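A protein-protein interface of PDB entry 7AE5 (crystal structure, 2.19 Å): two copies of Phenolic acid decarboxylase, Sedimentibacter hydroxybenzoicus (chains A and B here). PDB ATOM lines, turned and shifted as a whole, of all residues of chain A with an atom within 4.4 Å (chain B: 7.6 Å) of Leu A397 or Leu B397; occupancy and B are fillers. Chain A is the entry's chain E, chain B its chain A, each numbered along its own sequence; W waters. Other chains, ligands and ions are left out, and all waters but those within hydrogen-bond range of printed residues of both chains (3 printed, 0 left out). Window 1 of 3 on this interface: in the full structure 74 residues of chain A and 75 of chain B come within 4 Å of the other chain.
Tyr A347 touches Met B401, and with the chains exchanged Met A401 touches Tyr B347. Leu A397 touches its own counterpart, Leu B397. Leu A397 touches Glu B398, but with the chains exchanged Glu A398 does not touch Leu B397 (4.1 Å). Met A401 touches Leu B397, but with the chains exchanged Leu A397 does not touch Met B401 (4.3 Å). 10 positions are printed for both chains. Of the 6 pairs that touch across the chains among the printed residues, 3 have their exchanged pair printed and touching as well.
Water W2 bridges NE1 of Trp B314 (2.7 Å) and O of Glu A398 (3.1 Å). Water W3 lies within hydrogen-bond range of NZ of Lys B46 (2.7 Å) and O of Phe A395 (3.2 Å). Water W1 lies within hydrogen-bond range of the side-chain carboxylate (OE2) of Glu A398, the backbone NH (N) of Trp B314 and the side-chain amide nitrogen (ND2) of Asn A396.
Printed residues of chain A that touch a printed residue of chain B: Tyr A347, Leu A397, Glu A398 and Met A401. Hydrophobic or aromatic side chains of chain A that line the printed part of chain B: Tyr A347, Leu A397 and Met A401. Of the 19 printed residues of chain B, 5 touch a printed residue of chain A. Printed residues of chain B that touch a printed residue of chain A: Trp B314, Tyr B347, Leu B397, Glu B398 and Met B401. Hydrophobic or aromatic side chains of chain B that line the printed part of chain A: Trp B314, Tyr B347, Leu B397 and Met B401. Among the printed residues, 6 pairs touch across the chains. Among the printed residues, no Asp or Glu carboxylate lies within 4 Å of a Lys or Arg side-chain nitrogen of the other chain.
CD1 of Tyr A347 touches CB of Met B401 (3.8 Å). Leu A397 touches Leu B397. Glu B398 touches Leu A397 (N to CD1, 3.97 Å). Glu A398 touches Trp B314. CB of Met A401 touches CD1 of Tyr B347 (3.7 Å). CG of Met A401 touches CD1 of Leu B397, 3.99 Å away.
The side-chain amide oxygen of Asn A396 lies close to the backbone NH of Glu A398, 3.3 Å away. The side-chain amide nitrogen of Asn B344 is in hydrogen-bond range of the side-chain hydroxyl of Tyr B347, at 3.0 Å. OD1 of Asn B396 sits close to N of Glu B398.
Leu A397 touches two residues of chain B. Of the printed residues of chain B, Met A401 touches Tyr B347 and Leu B397. Printed residues of chain A within 4 Å of Trp B314: Glu A398. Printed residues of chain A within 4 Å of Leu B397: Leu A397 (3.5 Å) and Met A401 (3.99 Å). Of the printed residues of chain A, Met B401 touches Tyr A347. The nearest residue of chain B that does not touch Leu A397 is Met B401 (4.3 Å).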
ATOM      1  N   TYR A 347      20.816  19.329  16.116  1.00  0.00           N
ATOM      2  CA  TYR A 347      21.478  19.918  14.956  1.00  0.00           C
ATOM      3  C   TYR A 347      22.843  19.271  14.745  1.00  0.00           C
ATOM      4  O   TYR A 347      23.779  19.506  15.518  1.00  0.00           O
ATOM      5  CB  TYR A 347      21.579  21.431  15.132  1.00  0.00           C
ATOM      6  CG  TYR A 347      20.245  22.001  15.537  1.00  0.00           C
ATOM      7  CD1 TYR A 347      19.174  21.983  14.653  1.00  0.00           C
ATOM      8  CD2 TYR A 347      20.034  22.501  16.816  1.00  0.00           C
ATOM      9  CE1 TYR A 347      17.941  22.475  15.015  1.00  0.00           C
ATOM     10  CE2 TYR A 347      18.800  22.996  17.190  1.00  0.00           C
ATOM     11  CZ  TYR A 347      17.757  22.980  16.285  1.00  0.00           C
ATOM     12  OH  TYR A 347      16.523  23.470  16.646  1.00  0.00           O
ATOM     13  N   ILE A 354      20.671  23.599  22.300  1.00  0.00           N
ATOM     14  CA  ILE A 354      19.934  24.668  22.962  1.00  0.00           C
ATOM     15  C   ILE A 354      19.283  24.085  24.206  1.00  0.00           C
ATOM     16  O   ILE A 354      18.514  23.121  24.114  1.00  0.00           O
ATOM     17  CB  ILE A 354      18.881  25.307  22.044  1.00  0.00           C
ATOM     18  CG1 ILE A 354      19.510  25.678  20.701  1.00  0.00           C
ATOM     19  CG2 ILE A 354      18.263  26.531  22.708  1.00  0.00           C
ATOM     20  CD1 ILE A 354      18.534  26.245  19.711  1.00  0.00           C
ATOM     21  N   PRO A 394      13.059  25.603  23.823  1.00  0.00           N
ATOM     22  CA  PRO A 394      14.335  25.523  23.092  1.00  0.00           C
ATOM     23  C   PRO A 394      14.206  24.897  21.717  1.00  0.00           C
ATOM     24  O   PRO A 394      15.157  24.977  20.927  1.00  0.00           O
ATOM     25  CB  PRO A 394      15.206  24.666  24.013  1.00  0.00           C
ATOM     26  CG  PRO A 394      14.225  23.754  24.674  1.00  0.00           C
ATOM     27  CD  PRO A 394      12.978  24.591  24.892  1.00  0.00           C
ATOM     28  N   PHE A 395      13.072  24.273  21.412  1.00  0.00           N
ATOM     29  CA  PHE A 395      12.805  23.725  20.094  1.00  0.00           C
ATOM     30  C   PHE A 395      12.117  24.722  19.172  1.00  0.00           C
ATOM     31  O   PHE A 395      11.968  24.437  17.978  1.00  0.00           O
ATOM     32  CB  PHE A 395      11.949  22.461  20.219  1.00  0.00           C
ATOM     33  CG  PHE A 395      12.597  21.369  21.021  1.00  0.00           C
ATOM     34  CD1 PHE A 395      13.428  20.445  20.409  1.00  0.00           C
ATOM     35  CD2 PHE A 395      12.379  21.267  22.386  1.00  0.00           C
ATOM     36  CE1 PHE A 395      14.026  19.439  21.140  1.00  0.00           C
ATOM     37  CE2 PHE A 395      12.976  20.263  23.123  1.00  0.00           C
ATOM     38  CZ  PHE A 395      13.800  19.348  22.498  1.00  0.00           C
ATOM     39  N   ASN A 396      11.685  25.869  19.697  1.00  0.00           N
ATOM     40  CA  ASN A 396      11.068  26.930  18.903  1.00  0.00           C
ATOM     41  C   ASN A 396      12.158  27.952  18.599  1.00  0.00           C
ATOM     42  O   ASN A 396      12.480  28.802  19.435  1.00  0.00           O
ATOM     43  CB  ASN A 396       9.892  27.557  19.645  1.00  0.00           C
ATOM     44  CG  ASN A 396       9.040  28.443  18.750  1.00  0.00           C
ATOM     45  OD1 ASN A 396       9.553  29.165  17.894  1.00  0.00           O
ATOM     46  ND2 ASN A 396       7.727  28.386  18.944  1.00  0.00           N
ATOM     47  N   LEU A 397      12.724  27.870  17.396  1.00  0.00           N
ATOM     48  CA  LEU A 397      13.894  28.677  17.076  1.00  0.00           C
ATOM     49  C   LEU A 397      13.566  30.159  16.929  1.00  0.00           C
ATOM     50  O   LEU A 397      14.483  30.986  16.984  1.00  0.00           O
ATOM     51  CB  LEU A 397      14.558  28.143  15.806  1.00  0.00           C
ATOM     52  CG  LEU A 397      15.144  26.736  15.946  1.00  0.00           C
ATOM     53  CD1 LEU A 397      15.897  26.308  14.696  1.00  0.00           C
ATOM     54  CD2 LEU A 397      16.049  26.676  17.158  1.00  0.00           C
ATOM     55  N   GLU A 398      12.291  30.515  16.744  1.00  0.00           N
ATOM     56  CA  GLU A 398      11.910  31.923  16.804  1.00  0.00           C
ATOM     57  C   GLU A 398      12.049  32.459  18.223  1.00  0.00           C
ATOM     58  O   GLU A 398      12.588  33.550  18.439  1.00  0.00           O
ATOM     59  CB  GLU A 398      10.475  32.122  16.310  1.00  0.00           C
ATOM     60  CG  GLU A 398      10.158  31.550  14.944  1.00  0.00           C
ATOM     61  CD  GLU A 398       8.663  31.521  14.680  1.00  0.00           C
ATOM     62  OE1 GLU A 398       8.261  31.377  13.505  1.00  0.00           O
ATOM     63  OE2 GLU A 398       7.888  31.644  15.654  1.00  0.00           O
ATOM     64  N   GLN A 399      11.548  31.703  19.203  1.00  0.00           N
ATOM     65  CA  GLN A 399      11.682  32.107  20.598  1.00  0.00           C
ATOM     66  C   GLN A 399      13.140  32.139  21.029  1.00  0.00           C
ATOM     67  O   GLN A 399      13.527  32.980  21.846  1.00  0.00           O
ATOM     68  CB  GLN A 399      10.892  31.159  21.498  1.00  0.00           C
ATOM     69  CG  GLN A 399       9.398  31.407  21.518  1.00  0.00           C
ATOM     70  CD  GLN A 399       8.657  30.346  22.305  1.00  0.00           C
ATOM     71  OE1 GLN A 399       9.131  29.886  23.344  1.00  0.00           O
ATOM     72  NE2 GLN A 399       7.488  29.949  21.813  1.00  0.00           N
ATOM     73  N   VAL A 400      13.957  31.228  20.499  1.00  0.00           N
ATOM     74  CA  VAL A 400      15.384  31.256  20.798  1.00  0.00           C
ATOM     75  C   VAL A 400      16.025  32.501  20.200  1.00  0.00           C
ATOM     76  O   VAL A 400      16.882  33.135  20.828  1.00  0.00           O
ATOM     77  CB  VAL A 400      16.060  29.966  20.299  1.00  0.00           C
ATOM     78  CG1 VAL A 400      17.574  30.070  20.436  1.00  0.00           C
ATOM     79  CG2 VAL A 400      15.530  28.761  21.064  1.00  0.00           C
ATOM     80  N   MET A 401      15.613  32.880  18.986  1.00  0.00           N
ATOM     81  CA  MET A 401      16.101  34.127  18.407  1.00  0.00           C
ATOM     82  C   MET A 401      15.695  35.320  19.260  1.00  0.00           C
ATOM     83  O   MET A 401      16.479  36.259  19.438  1.00  0.00           O
ATOM     84  CB  MET A 401      15.586  34.297  16.976  1.00  0.00           C
ATOM     85  CG  MET A 401      16.301  33.436  15.951  1.00  0.00           C
ATOM     86  SD  MET A 401      18.062  33.789  15.736  1.00  0.00           S
ATOM     87  CE  MET A 401      18.147  35.568  15.964  1.00  0.00           C
ATOM     88  N   LYS B  46       2.502  26.700  14.217  1.00  0.00           N
ATOM     89  CA  LYS B  46       2.501  26.623  12.765  1.00  0.00           C
ATOM     90  C   LYS B  46       1.066  26.687  12.263  1.00  0.00           C
ATOM     91  O   LYS B  46       0.155  26.134  12.888  1.00  0.00           O
ATOM     92  CB  LYS B  46       3.188  25.329  12.256  1.00  0.00           C
ATOM     93  CG  LYS B  46       4.700  25.189  12.546  1.00  0.00           C
ATOM     94  CD  LYS B  46       5.062  25.063  14.028  1.00  0.00           C
ATOM     95  CE  LYS B  46       6.575  25.036  14.237  1.00  0.00           C
ATOM     96  NZ  LYS B  46       6.988  25.775  15.474  1.00  0.00           N
ATOM     97  N   TRP B 314       7.039  34.587  19.546  1.00  0.00           N
ATOM     98  CA  TRP B 314       6.396  35.346  18.474  1.00  0.00           C
ATOM     99  C   TRP B 314       4.886  35.487  18.676  1.00  0.00           C
ATOM    100  O   TRP B 314       4.216  34.544  19.099  1.00  0.00           O
ATOM    101  CB  TRP B 314       6.660  34.676  17.120  1.00  0.00           C
ATOM    102  CG  TRP B 314       7.904  35.137  16.415  1.00  0.00           C
ATOM    103  CD1 TRP B 314       9.142  35.312  16.960  1.00  0.00           C
ATOM    104  CD2 TRP B 314       8.027  35.469  15.025  1.00  0.00           C
ATOM    105  NE1 TRP B 314      10.027  35.736  15.999  1.00  0.00           N
ATOM    106  CE2 TRP B 314       9.368  35.842  14.802  1.00  0.00           C
ATOM    107  CE3 TRP B 314       7.133  35.490  13.949  1.00  0.00           C
ATOM    108  CZ2 TRP B 314       9.837  36.231  13.548  1.00  0.00           C
ATOM    109  CZ3 TRP B 314       7.599  35.878  12.706  1.00  0.00           C
ATOM    110  CH2 TRP B 314       8.939  36.245  12.516  1.00  0.00           C
ATOM    111  N   ASN B 344      17.349  38.231   6.092  1.00  0.00           N
ATOM    112  CA  ASN B 344      16.335  37.853   7.076  1.00  0.00           C
ATOM    113  C   ASN B 344      16.581  38.689   8.329  1.00  0.00           C
ATOM    114  O   ASN B 344      17.495  38.403   9.108  1.00  0.00           O
ATOM    115  CB  ASN B 344      16.399  36.351   7.360  1.00  0.00           C
ATOM    116  CG  ASN B 344      15.573  35.931   8.573  1.00  0.00           C
ATOM    117  OD1 ASN B 344      14.781  36.700   9.113  1.00  0.00           O
ATOM    118  ND2 ASN B 344      15.758  34.687   8.997  1.00  0.00           N
ATOM    119  N   MET B 346      13.936  39.490  10.688  1.00  0.00           N
ATOM    120  CA  MET B 346      12.599  39.423  11.264  1.00  0.00           C
ATOM    121  C   MET B 346      12.584  39.383  12.789  1.00  0.00           C
ATOM    122  O   MET B 346      11.496  39.365  13.376  1.00  0.00           O
ATOM    123  CB  MET B 346      11.859  38.189  10.738  1.00  0.00           C
ATOM    124  CG  MET B 346      11.996  37.938   9.250  1.00  0.00           C
ATOM    125  SD  MET B 346      10.838  36.676   8.693  1.00  0.00           S
ATOM    126  CE  MET B 346      11.700  35.188   9.199  1.00  0.00           C
ATOM    127  N   TYR B 347      13.739  39.374  13.446  1.00  0.00           N
ATOM    128  CA  TYR B 347      13.821  39.040  14.867  1.00  0.00           C
ATOM    129  C   TYR B 347      14.013  40.309  15.693  1.00  0.00           C
ATOM    130  O   TYR B 347      15.108  40.877  15.738  1.00  0.00           O
ATOM    131  CB  TYR B 347      14.933  38.019  15.087  1.00  0.00           C
ATOM    132  CG  TYR B 347      14.794  36.857  14.128  1.00  0.00           C
ATOM    133  CD1 TYR B 347      13.720  35.982  14.226  1.00  0.00           C
ATOM    134  CD2 TYR B 347      15.706  36.658  13.098  1.00  0.00           C
ATOM    135  CE1 TYR B 347      13.569  34.929  13.344  1.00  0.00           C
ATOM    136  CE2 TYR B 347      15.563  35.605  12.210  1.00  0.00           C
ATOM    137  CZ  TYR B 347      14.491  34.746  12.339  1.00  0.00           C
ATOM    138  OH  TYR B 347      14.338  33.697  11.462  1.00  0.00           O
ATOM    139  N   ILE B 354      20.045  37.522   9.570  1.00  0.00           N
ATOM    140  CA  ILE B 354      20.713  36.414   8.897  1.00  0.00           C
ATOM    141  C   ILE B 354      20.749  36.733   7.410  1.00  0.00           C
ATOM    142  O   ILE B 354      19.700  36.952   6.794  1.00  0.00           O
ATOM    143  CB  ILE B 354      20.010  35.069   9.149  1.00  0.00           C
ATOM    144  CG1 ILE B 354      19.863  34.819  10.651  1.00  0.00           C
ATOM    145  CG2 ILE B 354      20.788  33.935   8.503  1.00  0.00           C
ATOM    146  CD1 ILE B 354      18.797  33.815  10.992  1.00  0.00           C
ATOM    147  N   ILE B 386      24.395  36.976  11.307  1.00  0.00           N
ATOM    148  CA  ILE B 386      24.910  35.690  10.849  1.00  0.00           C
ATOM    149  C   ILE B 386      24.895  35.685   9.327  1.00  0.00           C
ATOM    150  O   ILE B 386      23.873  36.008   8.710  1.00  0.00           O
ATOM    151  CB  ILE B 386      24.079  34.522  11.410  1.00  0.00           C
ATOM    152  CG1 ILE B 386      24.043  34.576  12.941  1.00  0.00           C
ATOM    153  CG2 ILE B 386      24.626  33.190  10.917  1.00  0.00           C
ATOM    154  CD1 ILE B 386      23.031  33.631  13.567  1.00  0.00           C
ATOM    155  N   ASP B 393      18.916  28.770   2.845  1.00  0.00           N
ATOM    156  CA  ASP B 393      17.742  29.608   3.056  1.00  0.00           C
ATOM    157  C   ASP B 393      17.897  30.345   4.379  1.00  0.00           C
ATOM    158  O   ASP B 393      17.802  29.710   5.438  1.00  0.00           O
ATOM    159  CB  ASP B 393      16.467  28.756   3.051  1.00  0.00           C
ATOM    160  CG  ASP B 393      15.188  29.585   3.169  1.00  0.00           C
ATOM    161  OD1 ASP B 393      15.256  30.811   3.407  1.00  0.00           O
ATOM    162  OD2 ASP B 393      14.096  28.995   3.023  1.00  0.00           O
ATOM    163  N   PRO B 394      18.127  31.662   4.378  1.00  0.00           N
ATOM    164  CA  PRO B 394      18.294  32.375   5.653  1.00  0.00           C
ATOM    165  C   PRO B 394      17.027  32.419   6.488  1.00  0.00           C
ATOM    166  O   PRO B 394      17.105  32.723   7.685  1.00  0.00           O
ATOM    167  CB  PRO B 394      18.723  33.780   5.214  1.00  0.00           C
ATOM    168  CG  PRO B 394      18.128  33.936   3.855  1.00  0.00           C
ATOM    169  CD  PRO B 394      18.174  32.575   3.222  1.00  0.00           C
ATOM    170  N   PHE B 395      15.869  32.132   5.899  1.00  0.00           N
ATOM    171  CA  PHE B 395      14.612  32.065   6.630  1.00  0.00           C
ATOM    172  C   PHE B 395      14.318  30.670   7.164  1.00  0.00           C
ATOM    173  O   PHE B 395      13.259  30.462   7.767  1.00  0.00           O
ATOM    174  CB  PHE B 395      13.459  32.532   5.734  1.00  0.00           C
ATOM    175  CG  PHE B 395      13.596  33.952   5.262  1.00  0.00           C
ATOM    176  CD1 PHE B 395      13.189  35.005   6.063  1.00  0.00           C
ATOM    177  CD2 PHE B 395      14.142  34.233   4.021  1.00  0.00           C
ATOM    178  CE1 PHE B 395      13.319  36.314   5.633  1.00  0.00           C
ATOM    179  CE2 PHE B 395      14.273  35.538   3.583  1.00  0.00           C
ATOM    180  CZ  PHE B 395      13.862  36.580   4.391  1.00  0.00           C
ATOM    181  N   ASN B 396      15.220  29.716   6.953  1.00  0.00           N
ATOM    182  CA  ASN B 396      15.083  28.342   7.435  1.00  0.00           C
ATOM    183  C   ASN B 396      16.082  28.178   8.578  1.00  0.00           C
ATOM    184  O   ASN B 396      17.255  27.874   8.358  1.00  0.00           O
ATOM    185  CB  ASN B 396      15.332  27.341   6.304  1.00  0.00           C
ATOM    186  CG  ASN B 396      15.065  25.903   6.719  1.00  0.00           C
ATOM    187  OD1 ASN B 396      15.357  25.496   7.844  1.00  0.00           O
ATOM    188  ND2 ASN B 396      14.497  25.127   5.803  1.00  0.00           N
ATOM    189  N   LEU B 397      15.600  28.371   9.809  1.00  0.00           N
ATOM    190  CA  LEU B 397      16.496  28.405  10.960  1.00  0.00           C
ATOM    191  C   LEU B 397      17.165  27.059  11.205  1.00  0.00           C
ATOM    192  O   LEU B 397      18.265  27.008  11.768  1.00  0.00           O
ATOM    193  CB  LEU B 397      15.728  28.863  12.201  1.00  0.00           C
ATOM    194  CG  LEU B 397      15.239  30.311  12.135  1.00  0.00           C
ATOM    195  CD1 LEU B 397      14.676  30.768  13.469  1.00  0.00           C
ATOM    196  CD2 LEU B 397      16.373  31.221  11.701  1.00  0.00           C
ATOM    197  N   GLU B 398      16.529  25.959  10.793  1.00  0.00           N
ATOM    198  CA  GLU B 398      17.184  24.658  10.888  1.00  0.00           C
ATOM    199  C   GLU B 398      18.361  24.570   9.925  1.00  0.00           C
ATOM    200  O   GLU B 398      19.395  23.975  10.250  1.00  0.00           O
ATOM    201  CB  GLU B 398      16.181  23.537  10.614  1.00  0.00           C
ATOM    202  N   GLN B 399      18.218  25.152   8.733  1.00  0.00           N
ATOM    203  CA  GLN B 399      19.331  25.205   7.793  1.00  0.00           C
ATOM    204  C   GLN B 399      20.415  26.161   8.265  1.00  0.00           C
ATOM    205  O   GLN B 399      21.603  25.924   8.014  1.00  0.00           O
ATOM    206  CB  GLN B 399      18.830  25.619   6.411  1.00  0.00           C
ATOM    207  CG  GLN B 399      19.605  25.012   5.260  1.00  0.00           C
ATOM    208  CD  GLN B 399      18.829  25.062   3.960  1.00  0.00           C
ATOM    209  OE1 GLN B 399      18.851  26.068   3.251  1.00  0.00           O
ATOM    210  NE2 GLN B 399      18.128  23.976   3.643  1.00  0.00           N
ATOM    211  N   VAL B 400      20.030  27.244   8.941  1.00  0.00           N
ATOM    212  CA  VAL B 400      21.024  28.164   9.482  1.00  0.00           C
ATOM    213  C   VAL B 400      21.788  27.506  10.624  1.00  0.00           C
ATOM    214  O   VAL B 400      22.996  27.724  10.785  1.00  0.00           O
ATOM    215  CB  VAL B 400      20.350  29.477   9.921  1.00  0.00           C
ATOM    216  CG1 VAL B 400      21.364  30.411  10.570  1.00  0.00           C
ATOM    217  CG2 VAL B 400      19.691  30.152   8.725  1.00  0.00           C
ATOM    218  N   MET B 401      21.104  26.687  11.429  1.00  0.00           N
ATOM    219  CA  MET B 401      21.797  25.924  12.461  1.00  0.00           C
ATOM    220  C   MET B 401      22.842  25.002  11.850  1.00  0.00           C
ATOM    221  O   MET B 401      23.945  24.858  12.389  1.00  0.00           O
ATOM    222  CB  MET B 401      20.798  25.111  13.287  1.00  0.00           C
ATOM    223  CG  MET B 401      20.120  25.881  14.409  1.00  0.00           C
ATOM    224  SD  MET B 401      21.264  26.757  15.495  1.00  0.00           S
ATOM    225  CE  MET B 401      22.410  25.454  15.949  1.00  0.00           C
ATOM    226  N   TRP B 402      22.511  24.366  10.722  1.00  0.00           N
ATOM    227  CA  TRP B 402      23.470  23.492  10.056  1.00  0.00           C
ATOM    228  C   TRP B 402      24.709  24.266   9.625  1.00  0.00           C
ATOM    229  O   TRP B 402      25.841  23.809   9.821  1.00  0.00           O
ATOM    230  CB  TRP B 402      22.824  22.813   8.849  1.00  0.00           C
ATOM    231  CG  TRP B 402      23.837  22.139   7.976  1.00  0.00           C
ATOM    232  CD1 TRP B 402      24.494  20.973   8.236  1.00  0.00           C
ATOM    233  CD2 TRP B 402      24.335  22.608   6.718  1.00  0.00           C
ATOM    234  NE1 TRP B 402      25.359  20.678   7.212  1.00  0.00           N
ATOM    235  CE2 TRP B 402      25.283  21.667   6.268  1.00  0.00           C
ATOM    236  CE3 TRP B 402      24.069  23.730   5.926  1.00  0.00           C
ATOM    237  CZ2 TRP B 402      25.963  21.812   5.061  1.00  0.00           C
ATOM    238  CZ3 TRP B 402      24.747  23.873   4.729  1.00  0.00           C
ATOM    239  CH2 TRP B 402      25.682  22.919   4.308  1.00  0.00           C
ATOM    240  N   ALA B 403      24.511  25.444   9.028  1.00  0.00           N
ATOM    241  CA  ALA B 403      25.647  26.270   8.635  1.00  0.00           C
ATOM    242  C   ALA B 403      26.458  26.699   9.851  1.00  0.00           C
ATOM    243  O   ALA B 403      27.689  26.781   9.786  1.00  0.00           O
ATOM    244  CB  ALA B 403      25.164  27.490   7.851  1.00  0.00           C
ATOM    245  N   LEU B 404      25.788  26.972  10.971  1.00  0.00           N
ATOM    246  CA  LEU B 404      26.507  27.308  12.195  1.00  0.00           C
ATOM    247  C   LEU B 404      27.364  26.138  12.660  1.00  0.00           C
ATOM    248  O   LEU B 404      28.547  26.305  12.979  1.00  0.00           O
ATOM    249  CB  LEU B 404      25.521  27.714  13.293  1.00  0.00           C
ATOM    250  CG  LEU B 404      24.728  29.010  13.118  1.00  0.00           C
ATOM    251  CD1 LEU B 404      23.849  29.261  14.334  1.00  0.00           C
ATOM    252  CD2 LEU B 404      25.657  30.183  12.879  1.00  0.00           C
HETATM  253  O   HOH W   1       7.106  31.565  18.631  1.00  0.00           O
HETATM  254  O   HOH W   2      12.354  36.413  17.284  1.00  0.00           O
HETATM  255  O   HOH W   3       8.893  24.507  16.988  1.00  0.00           O
